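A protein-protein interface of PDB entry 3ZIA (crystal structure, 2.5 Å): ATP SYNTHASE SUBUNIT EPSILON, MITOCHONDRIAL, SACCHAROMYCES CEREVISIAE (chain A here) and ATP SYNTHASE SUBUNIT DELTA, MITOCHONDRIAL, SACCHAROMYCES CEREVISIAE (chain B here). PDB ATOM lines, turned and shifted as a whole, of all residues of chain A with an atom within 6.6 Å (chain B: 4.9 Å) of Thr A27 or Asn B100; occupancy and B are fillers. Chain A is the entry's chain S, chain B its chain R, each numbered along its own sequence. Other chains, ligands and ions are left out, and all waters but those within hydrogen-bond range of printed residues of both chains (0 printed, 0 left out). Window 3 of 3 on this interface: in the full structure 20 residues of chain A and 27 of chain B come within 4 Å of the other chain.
The side-chain amide nitrogen of Asn B100 lies within hydrogen-bond range of the backbone carbonyl oxygen of Leu A25, at 3.3 Å.
O of Ser A24 sits at hydrogen-bond distance from N of Ser B97 (3.3 Å).
NE2 of Gln A30 sits at hydrogen-bond distance from O of Ser A23, 3.1 Å away.
O of Leu A25 is in hydrogen-bond range of NE2 of Gln A30 (3.1 Å).
The side-chain amide nitrogen of Asn B100 lies within hydrogen-bond range of the side-chain hydroxyl of Ser B97 (2.8 Å).
Among the printed residues, pairs that only touch across the chains: Ser A24 with Leu B104 (3.5 Å), Ser A23 with Leu B104 (3.6 Å), Ser A24 with Ile B101 (3.6 Å), Lys A26 with Ser B97 (3.6 Å), Ser A23 with Asn B100 (3.7 Å), Leu A25 with Ser B97 (3.8 Å) and Thr A27 with Asn B100 (3.9 Å).
Printed residues of chain B within 4 Å of Ser A23: Asn B100 and Leu B104.
Of the printed residues of chain B, Lys A26 touches Ser B97 (3.6 Å).
Thr A27 touches one residue of chain B.
Of the printed residues of chain A, Ser B97 touches Ser A24 (3.3 Å), Leu A25 (3.8 Å) and Lys A26 (3.6 Å).
Glu B99 touches none of the printed residues of chain A.
Asn B100 touches just these residues of chain A: Ser A23, Leu A25 and Thr A27.
Of the printed residues of chain A, Ile B101 touches Ser A24.
Of the 9 printed residues of chain A, 5 touch a printed residue of chain B.
Printed residues of chain A that touch a printed residue of chain B: Ser A23, Ser A24, Leu A25, Lys A26 and Thr A27.
Of the 8 printed residues of chain B, 4 touch a printed residue of chain A.
Printed residues of chain B that touch a printed residue of chain A: Ser B97, Asn B100, Ile B101 and Leu B104.
Hydrophobic or aromatic side chains of chain B that line the printed part of chain A: Ile B101 and Leu B104.
Among the printed residues, no Asp or Glu carboxylate lies within 4 Å of a Lys or Arg side-chain nitrogen of the other chain.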
ATOM      1  N   SER A  23       7.679  21.061   8.627  1.00  0.00           N
ATOM      2  CA  SER A  23       6.451  20.392   9.074  1.00  0.00           C
ATOM      3  C   SER A  23       6.735  19.216  10.022  1.00  0.00           C
ATOM      4  O   SER A  23       5.877  18.847  10.830  1.00  0.00           O
ATOM      5  CB  SER A  23       5.633  19.897   7.878  1.00  0.00           C
ATOM      6  OG  SER A  23       5.305  20.944   6.988  1.00  0.00           O
ATOM      7  N   SER A  24       7.936  18.646   9.921  1.00  0.00           N
ATOM      8  CA  SER A  24       8.319  17.466  10.699  1.00  0.00           C
ATOM      9  C   SER A  24       8.715  17.781  12.138  1.00  0.00           C
ATOM     10  O   SER A  24       8.776  16.876  12.981  1.00  0.00           O
ATOM     11  CB  SER A  24       9.458  16.712  10.015  1.00  0.00           C
ATOM     12  OG  SER A  24       8.963  15.828   9.028  1.00  0.00           O
ATOM     13  N   LEU A  25       8.987  19.056  12.409  1.00  0.00           N
ATOM     14  CA  LEU A  25       9.421  19.502  13.729  1.00  0.00           C
ATOM     15  C   LEU A  25       8.388  19.195  14.802  1.00  0.00           C
ATOM     16  O   LEU A  25       7.203  19.023  14.496  1.00  0.00           O
ATOM     17  CB  LEU A  25       9.688  21.007  13.723  1.00  0.00           C
ATOM     18  CG  LEU A  25      10.907  21.536  12.981  1.00  0.00           C
ATOM     19  CD1 LEU A  25      10.704  23.010  12.690  1.00  0.00           C
ATOM     20  CD2 LEU A  25      12.186  21.302  13.784  1.00  0.00           C
ATOM     21  N   LYS A  26       8.843  19.125  16.055  1.00  0.00           N
ATOM     22  CA  LYS A  26       7.943  19.064  17.207  1.00  0.00           C
ATOM     23  C   LYS A  26       7.071  20.306  17.157  1.00  0.00           C
ATOM     24  O   LYS A  26       7.585  21.424  17.146  1.00  0.00           O
ATOM     25  CB  LYS A  26       8.724  19.024  18.523  1.00  0.00           C
ATOM     26  CG  LYS A  26       9.603  17.788  18.688  1.00  0.00           C
ATOM     27  CD  LYS A  26      10.496  17.869  19.912  1.00  0.00           C
ATOM     28  CE  LYS A  26       9.850  17.237  21.133  1.00  0.00           C
ATOM     29  NZ  LYS A  26      10.816  17.162  22.263  1.00  0.00           N
ATOM     30  N   THR A  27       5.757  20.102  17.100  1.00  0.00           N
ATOM     31  CA  THR A  27       4.802  21.193  16.864  1.00  0.00           C
ATOM     32  C   THR A  27       5.067  22.482  17.662  1.00  0.00           C
ATOM     33  O   THR A  27       4.940  23.576  17.114  1.00  0.00           O
ATOM     34  CB  THR A  27       3.312  20.723  16.992  1.00  0.00           C
ATOM     35  OG1 THR A  27       2.538  21.739  17.642  1.00  0.00           O
ATOM     36  CG2 THR A  27       3.191  19.411  17.780  1.00  0.00           C
ATOM     37  N   GLU A  28       5.452  22.354  18.932  1.00  0.00           N
ATOM     38  CA  GLU A  28       5.757  23.529  19.763  1.00  0.00           C
ATOM     39  C   GLU A  28       6.990  24.305  19.285  1.00  0.00           C
ATOM     40  O   GLU A  28       7.085  25.513  19.495  1.00  0.00           O
ATOM     41  CB  GLU A  28       5.884  23.161  21.252  1.00  0.00           C
ATOM     42  CG  GLU A  28       7.034  22.214  21.609  1.00  0.00           C
ATOM     43  CD  GLU A  28       6.625  20.743  21.622  1.00  0.00           C
ATOM     44  OE1 GLU A  28       5.641  20.374  20.940  1.00  0.00           O
ATOM     45  OE2 GLU A  28       7.296  19.952  22.320  1.00  0.00           O
ATOM     46  N   LEU A  29       7.924  23.609  18.641  1.00  0.00           N
ATOM     47  CA  LEU A  29       9.105  24.246  18.048  1.00  0.00           C
ATOM     48  C   LEU A  29       8.856  24.780  16.632  1.00  0.00           C
ATOM     49  O   LEU A  29       9.743  25.397  16.033  1.00  0.00           O
ATOM     50  CB  LEU A  29      10.311  23.295  18.062  1.00  0.00           C
ATOM     51  CG  LEU A  29      11.078  23.161  19.385  1.00  0.00           C
ATOM     52  CD1 LEU A  29      11.932  21.900  19.383  1.00  0.00           C
ATOM     53  CD2 LEU A  29      11.934  24.404  19.683  1.00  0.00           C
ATOM     54  N   GLN A  30       7.656  24.544  16.102  1.00  0.00           N
ATOM     55  CA  GLN A  30       7.227  25.174  14.851  1.00  0.00           C
ATOM     56  C   GLN A  30       6.787  26.610  15.139  1.00  0.00           C
ATOM     57  O   GLN A  30       5.604  26.952  15.020  1.00  0.00           O
ATOM     58  CB  GLN A  30       6.104  24.379  14.176  1.00  0.00           C
ATOM     59  CG  GLN A  30       6.563  23.092  13.505  1.00  0.00           C
ATOM     60  CD  GLN A  30       5.435  22.345  12.811  1.00  0.00           C
ATOM     61  OE1 GLN A  30       4.612  22.941  12.115  1.00  0.00           O
ATOM     62  NE2 GLN A  30       5.401  21.030  12.988  1.00  0.00           N
ATOM     63  N   THR A  31       7.760  27.440  15.517  1.00  0.00           N
ATOM     64  CA  THR A  31       7.522  28.823  15.939  1.00  0.00           C
ATOM     65  C   THR A  31       6.929  29.707  14.831  1.00  0.00           C
ATOM     66  O   THR A  31       6.882  29.315  13.656  1.00  0.00           O
ATOM     67  CB  THR A  31       8.799  29.468  16.587  1.00  0.00           C
ATOM     68  OG1 THR A  31       8.580  30.865  16.811  1.00  0.00           O
ATOM     69  CG2 THR A  31      10.032  29.298  15.713  1.00  0.00           C
ATOM     70  N   SER B  97       9.078  15.452  15.946  1.00  0.00           N
ATOM     71  CA  SER B  97       8.034  14.597  16.511  1.00  0.00           C
ATOM     72  C   SER B  97       7.689  13.482  15.526  1.00  0.00           C
ATOM     73  O   SER B  97       7.380  13.743  14.355  1.00  0.00           O
ATOM     74  CB  SER B  97       6.783  15.405  16.879  1.00  0.00           C
ATOM     75  OG  SER B  97       5.969  15.653  15.748  1.00  0.00           O
ATOM     76  N   GLN B  98       7.741  12.246  16.022  1.00  0.00           N
ATOM     77  CA  GLN B  98       7.582  11.041  15.202  1.00  0.00           C
ATOM     78  C   GLN B  98       6.308  11.062  14.357  1.00  0.00           C
ATOM     79  O   GLN B  98       6.343  10.758  13.161  1.00  0.00           O
ATOM     80  CB  GLN B  98       7.596   9.784  16.083  1.00  0.00           C
ATOM     81  CG  GLN B  98       8.762   9.688  17.080  1.00  0.00           C
ATOM     82  CD  GLN B  98      10.063   9.188  16.461  1.00  0.00           C
ATOM     83  OE1 GLN B  98      10.064   8.480  15.451  1.00  0.00           O
ATOM     84  NE2 GLN B  98      11.181   9.544  17.083  1.00  0.00           N
ATOM     85  N   GLU B  99       5.195  11.440  14.985  1.00  0.00           N
ATOM     86  CA  GLU B  99       3.871  11.366  14.356  1.00  0.00           C
ATOM     87  C   GLU B  99       3.644  12.358  13.215  1.00  0.00           C
ATOM     88  O   GLU B  99       3.004  12.015  12.215  1.00  0.00           O
ATOM     89  CB  GLU B  99       2.765  11.492  15.402  1.00  0.00           C
ATOM     90  CG  GLU B  99       3.012  12.552  16.452  1.00  0.00           C
ATOM     91  CD  GLU B  99       1.949  12.552  17.523  1.00  0.00           C
ATOM     92  OE1 GLU B  99       0.788  12.901  17.211  1.00  0.00           O
ATOM     93  OE2 GLU B  99       2.274  12.204  18.680  1.00  0.00           O
ATOM     94  N   ASN B 100       4.159  13.577  13.366  1.00  0.00           N
ATOM     95  CA  ASN B 100       4.090  14.573  12.298  1.00  0.00           C
ATOM     96  C   ASN B 100       4.766  14.065  11.037  1.00  0.00           C
ATOM     97  O   ASN B 100       4.255  14.251   9.934  1.00  0.00           O
ATOM     98  CB  ASN B 100       4.701  15.902  12.741  1.00  0.00           C
ATOM     99  CG  ASN B 100       3.741  16.739  13.561  1.00  0.00           C
ATOM    100  OD1 ASN B 100       2.530  16.719  13.331  1.00  0.00           O
ATOM    101  ND2 ASN B 100       4.276  17.485  14.521  1.00  0.00           N
ATOM    102  N   ILE B 101       5.905  13.400  11.223  1.00  0.00           N
ATOM    103  CA  ILE B 101       6.638  12.769  10.132  1.00  0.00           C
ATOM    104  C   ILE B 101       5.769  11.701   9.458  1.00  0.00           C
ATOM    105  O   ILE B 101       5.728  11.609   8.230  1.00  0.00           O
ATOM    106  CB  ILE B 101       7.973  12.153  10.625  1.00  0.00           C
ATOM    107  CG1 ILE B 101       8.744  13.160  11.482  1.00  0.00           C
ATOM    108  CG2 ILE B 101       8.823  11.687   9.444  1.00  0.00           C
ATOM    109  CD1 ILE B 101       9.975  12.594  12.156  1.00  0.00           C
ATOM    110  N   LYS B 102       5.066  10.916  10.273  1.00  0.00           N
ATOM    111  CA  LYS B 102       4.183   9.864   9.770  1.00  0.00           C
ATOM    112  C   LYS B 102       3.007  10.440   8.989  1.00  0.00           C
ATOM    113  O   LYS B 102       2.743  10.007   7.863  1.00  0.00           O
ATOM    114  CB  LYS B 102       3.679   8.969  10.911  1.00  0.00           C
ATOM    115  CG  LYS B 102       4.729   8.036  11.502  1.00  0.00           C
ATOM    116  CD  LYS B 102       4.189   7.325  12.734  1.00  0.00           C
ATOM    117  CE  LYS B 102       5.314   6.717  13.563  1.00  0.00           C
ATOM    118  NZ  LYS B 102       4.886   6.475  14.968  1.00  0.00           N
ATOM    119  N   ASN B 103       2.316  11.415   9.584  1.00  0.00           N
ATOM    120  CA  ASN B 103       1.181  12.079   8.934  1.00  0.00           C
ATOM    121  C   ASN B 103       1.541  12.668   7.569  1.00  0.00           C
ATOM    122  O   ASN B 103       0.724  12.660   6.642  1.00  0.00           O
ATOM    123  CB  ASN B 103       0.584  13.167   9.835  1.00  0.00           C
ATOM    124  CG  ASN B 103      -0.330  12.602  10.909  1.00  0.00           C
ATOM    125  OD1 ASN B 103       0.114  12.273  12.011  1.00  0.00           O
ATOM    126  ND2 ASN B 103      -1.618  12.500  10.597  1.00  0.00           N
ATOM    127  N   LEU B 104       2.769  13.173   7.462  1.00  0.00           N
ATOM    128  CA  LEU B 104       3.305  13.699   6.211  1.00  0.00           C
ATOM    129  C   LEU B 104       3.643  12.559   5.259  1.00  0.00           C
ATOM    130  O   LEU B 104       3.225  12.569   4.096  1.00  0.00           O
ATOM    131  CB  LEU B 104       4.558  14.537   6.482  1.00  0.00           C
ATOM    132  CG  LEU B 104       4.514  16.007   6.910  1.00  0.00           C
ATOM    133  CD1 LEU B 104       3.230  16.433   7.638  1.00  0.00           C
ATOM    134  CD2 LEU B 104       5.742  16.283   7.766  1.00  0.00           C
